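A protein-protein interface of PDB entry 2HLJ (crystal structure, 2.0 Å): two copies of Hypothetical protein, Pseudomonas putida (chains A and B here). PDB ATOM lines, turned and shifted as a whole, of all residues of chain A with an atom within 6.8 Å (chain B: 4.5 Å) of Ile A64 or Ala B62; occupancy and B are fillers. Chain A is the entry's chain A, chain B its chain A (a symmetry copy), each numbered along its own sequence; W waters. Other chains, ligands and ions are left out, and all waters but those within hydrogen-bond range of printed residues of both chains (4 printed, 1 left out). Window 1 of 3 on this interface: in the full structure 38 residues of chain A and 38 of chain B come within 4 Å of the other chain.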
ATOM      1  N   ASP A  25     -13.190   3.420  17.165  1.00  0.00           N
ATOM      2  CA  ASP A  25     -12.560   2.939  18.395  1.00  0.00           C
ATOM      3  C   ASP A  25     -13.489   2.045  19.223  1.00  0.00           C
ATOM      4  O   ASP A  25     -13.075   0.978  19.706  1.00  0.00           O
ATOM      5  CB  ASP A  25     -12.042   4.117  19.272  1.00  0.00           C
ATOM      6  CG  ASP A  25     -13.108   5.220  19.545  1.00  0.00           C
ATOM      7  OD1 ASP A  25     -14.327   5.108  19.184  1.00  0.00           O
ATOM      8  OD2 ASP A  25     -12.684   6.243  20.099  1.00  0.00           O
ATOM      9  N   TYR A  28     -13.843  -1.670  18.008  1.00  0.00           N
ATOM     10  CA  TYR A  28     -12.780  -2.631  18.406  1.00  0.00           C
ATOM     11  C   TYR A  28     -13.208  -3.273  19.728  1.00  0.00           C
ATOM     12  O   TYR A  28     -13.170  -4.496  19.875  1.00  0.00           O
ATOM     13  CB  TYR A  28     -11.449  -1.966  18.656  1.00  0.00           C
ATOM     14  CG  TYR A  28     -10.649  -1.373  17.520  1.00  0.00           C
ATOM     15  CD1 TYR A  28     -10.996  -0.160  16.964  1.00  0.00           C
ATOM     16  CD2 TYR A  28      -9.446  -1.965  17.101  1.00  0.00           C
ATOM     17  CE1 TYR A  28     -10.232   0.407  15.983  1.00  0.00           C
ATOM     18  CE2 TYR A  28      -8.656  -1.393  16.123  1.00  0.00           C
ATOM     19  CZ  TYR A  28      -9.056  -0.191  15.564  1.00  0.00           C
ATOM     20  OH  TYR A  28      -8.294   0.431  14.583  1.00  0.00           O
ATOM     21  N   LEU A  29     -13.656  -2.440  20.675  1.00  0.00           N
ATOM     22  CA  LEU A  29     -14.168  -2.931  21.965  1.00  0.00           C
ATOM     23  C   LEU A  29     -15.429  -3.783  21.849  1.00  0.00           C
ATOM     24  O   LEU A  29     -15.580  -4.729  22.603  1.00  0.00           O
ATOM     25  CB  LEU A  29     -14.352  -1.795  22.985  1.00  0.00           C
ATOM     26  CG  LEU A  29     -14.344  -2.183  24.466  1.00  0.00           C
ATOM     27  CD1 LEU A  29     -12.955  -2.653  24.972  1.00  0.00           C
ATOM     28  CD2 LEU A  29     -14.811  -0.984  25.331  1.00  0.00           C
ATOM     29  N   PHE A  32     -14.213  -7.208  20.851  1.00  0.00           N
ATOM     30  CA  PHE A  32     -13.749  -7.856  22.077  1.00  0.00           C
ATOM     31  C   PHE A  32     -14.873  -8.290  23.055  1.00  0.00           C
ATOM     32  O   PHE A  32     -14.759  -9.346  23.695  1.00  0.00           O
ATOM     33  CB  PHE A  32     -12.721  -6.977  22.818  1.00  0.00           C
ATOM     34  CG  PHE A  32     -11.431  -6.731  22.079  1.00  0.00           C
ATOM     35  CD1 PHE A  32     -10.862  -7.671  21.227  1.00  0.00           C
ATOM     36  CD2 PHE A  32     -10.693  -5.573  22.364  1.00  0.00           C
ATOM     37  CE1 PHE A  32      -9.638  -7.425  20.616  1.00  0.00           C
ATOM     38  CE2 PHE A  32      -9.526  -5.298  21.708  1.00  0.00           C
ATOM     39  CZ  PHE A  32      -8.965  -6.233  20.863  1.00  0.00           C
ATOM     40  N   ALA A  62     -11.520  -1.518  31.793  1.00  0.00           N
ATOM     41  CA  ALA A  62     -10.787  -1.978  30.640  1.00  0.00           C
ATOM     42  C   ALA A  62      -9.819  -0.911  30.175  1.00  0.00           C
ATOM     43  O   ALA A  62     -10.096   0.299  30.285  1.00  0.00           O
ATOM     44  CB  ALA A  62     -11.753  -2.342  29.492  1.00  0.00           C
ATOM     45  N   HIS A  63      -8.665  -1.366  29.688  1.00  0.00           N
ATOM     46  CA  HIS A  63      -7.731  -0.507  28.968  1.00  0.00           C
ATOM     47  C   HIS A  63      -7.733  -1.005  27.537  1.00  0.00           C
ATOM     48  O   HIS A  63      -7.927  -2.187  27.309  1.00  0.00           O
ATOM     49  CB  HIS A  63      -6.308  -0.595  29.540  1.00  0.00           C
ATOM     50  CG  HIS A  63      -5.476   0.621  29.252  1.00  0.00           C
ATOM     51  ND1 HIS A  63      -4.530   0.637  28.261  1.00  0.00           N
ATOM     52  CD2 HIS A  63      -5.489   1.869  29.775  1.00  0.00           C
ATOM     53  CE1 HIS A  63      -3.994   1.838  28.188  1.00  0.00           C
ATOM     54  NE2 HIS A  63      -4.559   2.607  29.093  1.00  0.00           N
ATOM     55  N   ILE A  64      -7.544  -0.116  26.572  1.00  0.00           N
ATOM     56  CA  ILE A  64      -7.378  -0.560  25.213  1.00  0.00           C
ATOM     57  C   ILE A  64      -6.334   0.257  24.502  1.00  0.00           C
ATOM     58  O   ILE A  64      -6.323   1.486  24.573  1.00  0.00           O
ATOM     59  CB  ILE A  64      -8.732  -0.627  24.447  1.00  0.00           C
ATOM     60  CG1 ILE A  64      -8.495  -0.975  22.997  1.00  0.00           C
ATOM     61  CG2 ILE A  64      -9.489   0.639  24.528  1.00  0.00           C
ATOM     62  CD1 ILE A  64      -9.773  -1.445  22.366  1.00  0.00           C
ATOM     63  N   ASN A  65      -5.413  -0.455  23.867  1.00  0.00           N
ATOM     64  CA  ASN A  65      -4.417   0.166  23.007  1.00  0.00           C
ATOM     65  C   ASN A  65      -4.746  -0.089  21.576  1.00  0.00           C
ATOM     66  O   ASN A  65      -4.929  -1.240  21.204  1.00  0.00           O
ATOM     67  CB  ASN A  65      -3.068  -0.414  23.310  1.00  0.00           C
ATOM     68  CG  ASN A  65      -2.638  -0.077  24.698  1.00  0.00           C
ATOM     69  OD1 ASN A  65      -3.068  -0.715  25.660  1.00  0.00           O
ATOM     70  ND2 ASN A  65      -1.848   0.973  24.826  1.00  0.00           N
ATOM     71  N   TYR A  66      -4.742   0.963  20.760  1.00  0.00           N
ATOM     72  CA  TYR A  66      -5.035   0.817  19.335  1.00  0.00           C
ATOM     73  C   TYR A  66      -3.743   1.052  18.567  1.00  0.00           C
ATOM     74  O   TYR A  66      -3.223   2.156  18.587  1.00  0.00           O
ATOM     75  CB  TYR A  66      -6.074   1.839  18.901  1.00  0.00           C
ATOM     76  CG  TYR A  66      -7.363   1.821  19.683  1.00  0.00           C
ATOM     77  CD1 TYR A  66      -7.528   2.618  20.826  1.00  0.00           C
ATOM     78  CD2 TYR A  66      -8.471   1.111  19.217  1.00  0.00           C
ATOM     79  CE1 TYR A  66      -8.724   2.641  21.507  1.00  0.00           C
ATOM     80  CE2 TYR A  66      -9.656   1.152  19.882  1.00  0.00           C
ATOM     81  CZ  TYR A  66      -9.784   1.893  21.028  1.00  0.00           C
ATOM     82  OH  TYR A  66     -11.006   1.889  21.670  1.00  0.00           O
ATOM     83  N   ALA A 106      -4.841  -4.283  17.815  1.00  0.00           N
ATOM     84  CA  ALA A 106      -5.289  -3.683  19.068  1.00  0.00           C
ATOM     85  C   ALA A 106      -5.242  -4.754  20.140  1.00  0.00           C
ATOM     86  O   ALA A 106      -5.224  -5.942  19.828  1.00  0.00           O
ATOM     87  CB  ALA A 106      -6.713  -3.184  18.937  1.00  0.00           C
ATOM     88  N   ALA A 107      -5.217  -4.324  21.392  1.00  0.00           N
ATOM     89  CA  ALA A 107      -5.203  -5.225  22.565  1.00  0.00           C
ATOM     90  C   ALA A 107      -5.970  -4.562  23.717  1.00  0.00           C
ATOM     91  O   ALA A 107      -6.003  -3.314  23.819  1.00  0.00           O
ATOM     92  CB  ALA A 107      -3.757  -5.534  22.956  1.00  0.00           C
ATOM     93  N   SER A 108      -6.587  -5.362  24.587  1.00  0.00           N
ATOM     94  CA  SER A 108      -7.323  -4.824  25.716  1.00  0.00           C
ATOM     95  C   SER A 108      -7.196  -5.718  26.906  1.00  0.00           C
ATOM     96  O   SER A 108      -7.453  -6.917  26.796  1.00  0.00           O
ATOM     97  CB  SER A 108      -8.824  -4.726  25.371  1.00  0.00           C
ATOM     98  OG  SER A 108      -9.513  -4.114  26.438  1.00  0.00           O
ATOM     99  N   GLU A 109      -6.845  -5.119  28.050  1.00  0.00           N
ATOM    100  CA  GLU A 109      -6.812  -5.778  29.336  1.00  0.00           C
ATOM    101  C   GLU A 109      -8.100  -5.418  30.039  1.00  0.00           C
ATOM    102  O   GLU A 109      -8.458  -4.250  30.062  1.00  0.00           O
ATOM    103  CB  GLU A 109      -5.622  -5.225  30.151  1.00  0.00           C
ATOM    104  CG  GLU A 109      -5.370  -5.982  31.445  1.00  0.00           C
ATOM    105  CD  GLU A 109      -4.353  -5.309  32.345  1.00  0.00           C
ATOM    106  OE1 GLU A 109      -3.838  -4.222  31.970  1.00  0.00           O
ATOM    107  OE2 GLU A 109      -4.057  -5.879  33.424  1.00  0.00           O
ATOM    108  N   GLN A 110      -8.801  -6.396  30.614  1.00  0.00           N
ATOM    109  CA  GLN A 110     -10.080  -6.135  31.226  1.00  0.00           C
ATOM    110  C   GLN A 110     -10.253  -6.899  32.490  1.00  0.00           C
ATOM    111  O   GLN A 110      -9.709  -7.997  32.641  1.00  0.00           O
ATOM    112  CB  GLN A 110     -11.222  -6.560  30.299  1.00  0.00           C
ATOM    113  CG  GLN A 110     -10.961  -6.205  28.858  1.00  0.00           C
ATOM    114  CD  GLN A 110     -12.199  -6.246  28.043  1.00  0.00           C
ATOM    115  OE1 GLN A 110     -13.152  -6.942  28.380  1.00  0.00           O
ATOM    116  NE2 GLN A 110     -12.198  -5.512  26.954  1.00  0.00           N
ATOM    117  N   TYR A 148       0.404  -5.434  26.340  1.00  0.00           N
ATOM    118  CA  TYR A 148      -0.292  -4.194  26.720  1.00  0.00           C
ATOM    119  C   TYR A 148      -1.044  -4.382  28.039  1.00  0.00           C
ATOM    120  O   TYR A 148      -2.281  -4.492  28.102  1.00  0.00           O
ATOM    121  CB  TYR A 148      -1.197  -3.740  25.556  1.00  0.00           C
ATOM    122  CG  TYR A 148      -0.350  -3.424  24.341  1.00  0.00           C
ATOM    123  CD1 TYR A 148       0.216  -2.176  24.170  1.00  0.00           C
ATOM    124  CD2 TYR A 148      -0.078  -4.395  23.388  1.00  0.00           C
ATOM    125  CE1 TYR A 148       1.030  -1.900  23.082  1.00  0.00           C
ATOM    126  CE2 TYR A 148       0.718  -4.114  22.281  1.00  0.00           C
ATOM    127  CZ  TYR A 148       1.275  -2.877  22.158  1.00  0.00           C
ATOM    128  OH  TYR A 148       2.056  -2.628  21.084  1.00  0.00           O
ATOM    129  N   ILE A 153      -1.782   6.383  30.482  1.00  0.00           N
ATOM    130  CA  ILE A 153      -1.801   7.346  29.404  1.00  0.00           C
ATOM    131  C   ILE A 153      -0.981   8.538  29.814  1.00  0.00           C
ATOM    132  O   ILE A 153      -1.071   8.986  30.953  1.00  0.00           O
ATOM    133  CB  ILE A 153      -3.249   7.808  29.122  1.00  0.00           C
ATOM    134  CG1 ILE A 153      -4.059   6.665  28.496  1.00  0.00           C
ATOM    135  CG2 ILE A 153      -3.256   8.992  28.211  1.00  0.00           C
ATOM    136  CD1 ILE A 153      -5.588   6.793  28.670  1.00  0.00           C
ATOM    137  N   LEU B  60      -5.650   6.539  20.173  1.00  0.00           N
ATOM    138  CA  LEU B  60      -4.429   5.777  20.414  1.00  0.00           C
ATOM    139  C   LEU B  60      -4.634   4.757  21.541  1.00  0.00           C
ATOM    140  O   LEU B  60      -4.145   3.637  21.467  1.00  0.00           O
ATOM    141  CB  LEU B  60      -3.271   6.709  20.781  1.00  0.00           C
ATOM    142  CG  LEU B  60      -2.752   7.590  19.655  1.00  0.00           C
ATOM    143  CD1 LEU B  60      -1.765   8.606  20.175  1.00  0.00           C
ATOM    144  CD2 LEU B  60      -2.147   6.715  18.583  1.00  0.00           C
ATOM    145  N   GLU B  61      -5.386   5.165  22.555  1.00  0.00           N
ATOM    146  CA  GLU B  61      -5.400   4.484  23.840  1.00  0.00           C
ATOM    147  C   GLU B  61      -6.542   5.040  24.669  1.00  0.00           C
ATOM    148  O   GLU B  61      -6.811   6.235  24.634  1.00  0.00           O
ATOM    149  CB  GLU B  61      -4.074   4.771  24.548  1.00  0.00           C
ATOM    150  CG  GLU B  61      -3.721   3.865  25.687  1.00  0.00           C
ATOM    151  CD  GLU B  61      -2.325   4.136  26.237  1.00  0.00           C
ATOM    152  OE1 GLU B  61      -1.565   4.984  25.691  1.00  0.00           O
ATOM    153  OE2 GLU B  61      -1.974   3.467  27.214  1.00  0.00           O
ATOM    154  N   ALA B  62      -7.195   4.181  25.441  1.00  0.00           N
ATOM    155  CA  ALA B  62      -8.253   4.592  26.329  1.00  0.00           C
ATOM    156  C   ALA B  62      -8.333   3.658  27.516  1.00  0.00           C
ATOM    157  O   ALA B  62      -8.066   2.446  27.400  1.00  0.00           O
ATOM    158  CB  ALA B  62      -9.607   4.611  25.587  1.00  0.00           C
ATOM    159  N   HIS B  63      -8.669   4.234  28.670  1.00  0.00           N
ATOM    160  CA  HIS B  63      -9.039   3.459  29.849  1.00  0.00           C
ATOM    161  C   HIS B  63     -10.511   3.738  30.081  1.00  0.00           C
ATOM    162  O   HIS B  63     -10.976   4.822  29.771  1.00  0.00           O
ATOM    163  CB  HIS B  63      -8.237   3.878  31.091  1.00  0.00           C
ATOM    164  CG  HIS B  63      -8.144   2.800  32.131  1.00  0.00           C
ATOM    165  ND1 HIS B  63      -8.923   2.808  33.259  1.00  0.00           N
ATOM    166  CD2 HIS B  63      -7.421   1.657  32.187  1.00  0.00           C
ATOM    167  CE1 HIS B  63      -8.682   1.724  33.964  1.00  0.00           C
ATOM    168  NE2 HIS B  63      -7.776   1.005  33.336  1.00  0.00           N
ATOM    169  N   ILE B  64     -11.251   2.767  30.597  1.00  0.00           N
ATOM    170  CA  ILE B  64     -12.612   3.033  30.982  1.00  0.00           C
ATOM    171  C   ILE B  64     -12.960   2.320  32.260  1.00  0.00           C
ATOM    172  O   ILE B  64     -12.672   1.134  32.432  1.00  0.00           O
ATOM    173  CB  ILE B  64     -13.617   2.749  29.827  1.00  0.00           C
ATOM    174  CG1 ILE B  64     -15.035   2.921  30.315  1.00  0.00           C
ATOM    175  CG2 ILE B  64     -13.456   1.394  29.260  1.00  0.00           C
ATOM    176  CD1 ILE B  64     -15.967   3.062  29.147  1.00  0.00           C
ATOM    177  N   SER B 108     -13.917   7.758  31.190  1.00  0.00           N
ATOM    178  CA  SER B 108     -12.868   7.266  30.316  1.00  0.00           C
ATOM    179  C   SER B 108     -11.852   8.331  30.056  1.00  0.00           C
ATOM    180  O   SER B 108     -12.219   9.437  29.659  1.00  0.00           O
ATOM    181  CB  SER B 108     -13.465   6.857  28.952  1.00  0.00           C
ATOM    182  OG  SER B 108     -12.454   6.292  28.147  1.00  0.00           O
ATOM    183  N   GLU B 109     -10.575   7.974  30.238  1.00  0.00           N
ATOM    184  CA  GLU B 109      -9.443   8.807  29.901  1.00  0.00           C
ATOM    185  C   GLU B 109      -8.940   8.329  28.559  1.00  0.00           C
ATOM    186  O   GLU B 109      -8.779   7.133  28.375  1.00  0.00           O
ATOM    187  CB  GLU B 109      -8.336   8.595  30.957  1.00  0.00           C
ATOM    188  CG  GLU B 109      -7.171   9.563  30.816  1.00  0.00           C
ATOM    189  CD  GLU B 109      -5.993   9.217  31.704  1.00  0.00           C
ATOM    190  OE1 GLU B 109      -6.068   8.196  32.438  1.00  0.00           O
ATOM    191  OE2 GLU B 109      -4.996   9.980  31.679  1.00  0.00           O
ATOM    192  N   GLN B 110      -8.689   9.241  27.618  1.00  0.00           N
ATOM    193  CA  GLN B 110      -8.290   8.848  26.289  1.00  0.00           C
ATOM    194  C   GLN B 110      -7.235   9.744  25.743  1.00  0.00           C
ATOM    195  O   GLN B 110      -7.182  10.931  26.078  1.00  0.00           O
ATOM    196  CB  GLN B 110      -9.474   8.928  25.322  1.00  0.00           C
ATOM    197  CG  GLN B 110     -10.754   8.421  25.931  1.00  0.00           C
ATOM    198  CD  GLN B 110     -11.781   8.125  24.903  1.00  0.00           C
ATOM    199  OE1 GLN B 110     -11.756   8.683  23.810  1.00  0.00           O
ATOM    200  NE2 GLN B 110     -12.703   7.254  25.241  1.00  0.00           N
HETATM  201  O   HOH W   1     -13.467   8.646  21.838  1.00  0.00           O
HETATM  202  O   HOH W   2      -1.470   3.217  20.463  1.00  0.00           O
HETATM  203  O   HOH W   3     -14.357   6.453  23.047  1.00  0.00           O
HETATM  204  O   HOH W   4      -2.960   9.578  33.174  1.00  0.00           O
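O of Ala B62 is in hydrogen-bond range of N of Ile A64 (2.7 Å).
ND2 of Asn A65 is in hydrogen-bond range of OE2 of Glu B61 (3.5 Å).
The backbone carbonyl oxygen of Ala A62 lies within hydrogen-bond range of the backbone NH of Ile B64, at 2.7 Å.
A ring nitrogen (NE2) of His A63 lies close to the side-chain carboxylate (OE2) of Glu B61 (3.3 Å).
The backbone NH (N) of Tyr A66 lies within hydrogen-bond range of the backbone carbonyl oxygen (O) of Leu B60, 2.8 Å away.
A ring nitrogen (ND1) of His A63 is in hydrogen-bond range of the side-chain amide oxygen (OD1) of Asn A65 (3.3 Å).
The side-chain hydroxyl (OG) of Ser B108 sits at hydrogen-bond distance from the backbone carbonyl oxygen (O) of His B63 (2.6 Å).
The backbone NH (N) of His B63 sits at hydrogen-bond distance from the backbone carbonyl oxygen (O) of Glu B109, 2.9 Å away.
The side-chain hydroxyl of Ser A108 lies within hydrogen-bond range of the backbone carbonyl oxygen of His A63, at 2.6 Å.
The backbone carbonyl oxygen (O) of Ala A107 sits at hydrogen-bond distance from the backbone NH (N) of Asn A65 (2.9 Å).
The backbone NH of His A63 lies within hydrogen-bond range of the backbone carbonyl oxygen of Glu A109.
Among the printed residues, pairs that only touch across the chains: Ala A62 with His B63 (3.4 Å), His A63 with Ala B62 (3.4 Å), His A63 with His B63 (3.1 Å), Ile A64 with Glu B61 (3.2 Å), Asn A65 with Leu B60 (3.8 Å), Tyr A66 with Glu B61 (3.8 Å), Ile A153 with Glu B61 (3.8 Å) and Ile A153 with Glu B109 (3.2 Å).
Of the printed residues of chain B, Ala A62 touches His B63 and Ile B64.
Ile A64 touches just these residues of chain B: Glu B61 and Ala B62.
Of the printed residues of chain B, Tyr A66 touches Leu B60 and Glu B61.
Printed residues of chain A within 4 Å of Leu B60: Asn A65 (3.8 Å) and Tyr A66 (2.8 Å).
Ala B62 touches two residues of chain A.
Printed residues of chain A within 4 Å of His B63: Ala A62 (3.4 Å) and His A63 (3.1 Å).
The nearest residue of chain A that does not touch Ala B62 is Ala A62 (4.1 Å).
Of the 8 printed residues of chain B, 6 touch a printed residue of chain A.
Printed residues of chain B that touch a printed residue of chain A: Leu B60, Glu B61, Ala B62, His B63, Ile B64 and Glu B109.
Hydrophobic or aromatic side chains of chain B within 4 Å of the printed part of chain A: His B63 and Ile B64.
Hydrophobic or aromatic side chains of chain A within 4 Å of the printed part of chain B: His A63, Ile A64, Tyr A66 and Ile A153.
Among the printed residues, 13 pairs touch across the chains.
Among the printed residues, no Asp or Glu carboxylate lies within 4 Å of a Lys or Arg side-chain nitrogen of the other chain.
Ala A62 touches His B63, and with the chains exchanged His A63 touches Ala B62.
Ala A62 touches Ile B64, and with the chains exchanged Ile A64 touches Ala B62.
His A63 touches its own counterpart, His B63.
Positions printed for both chains: 62, 63, 64, 108, 109 and 110.
Of the 13 pairs that touch across the chains among the printed residues, 5 have their exchanged pair printed and touching as well.
Water W4 bridges OE2 of Glu B109 (2.6 Å) and O of Ile A153 (3.0 Å).
Water W1 bridges the side-chain amide oxygen of Gln B110 and the side-chain carboxylate of Asp A25.
Water W2 bridges O of Tyr A66 (2.8 Å) and O of Leu B60 (2.9 Å).
Water W3 lies within hydrogen-bond range of NE2 of Gln B110 and OD2 of Asp A25.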
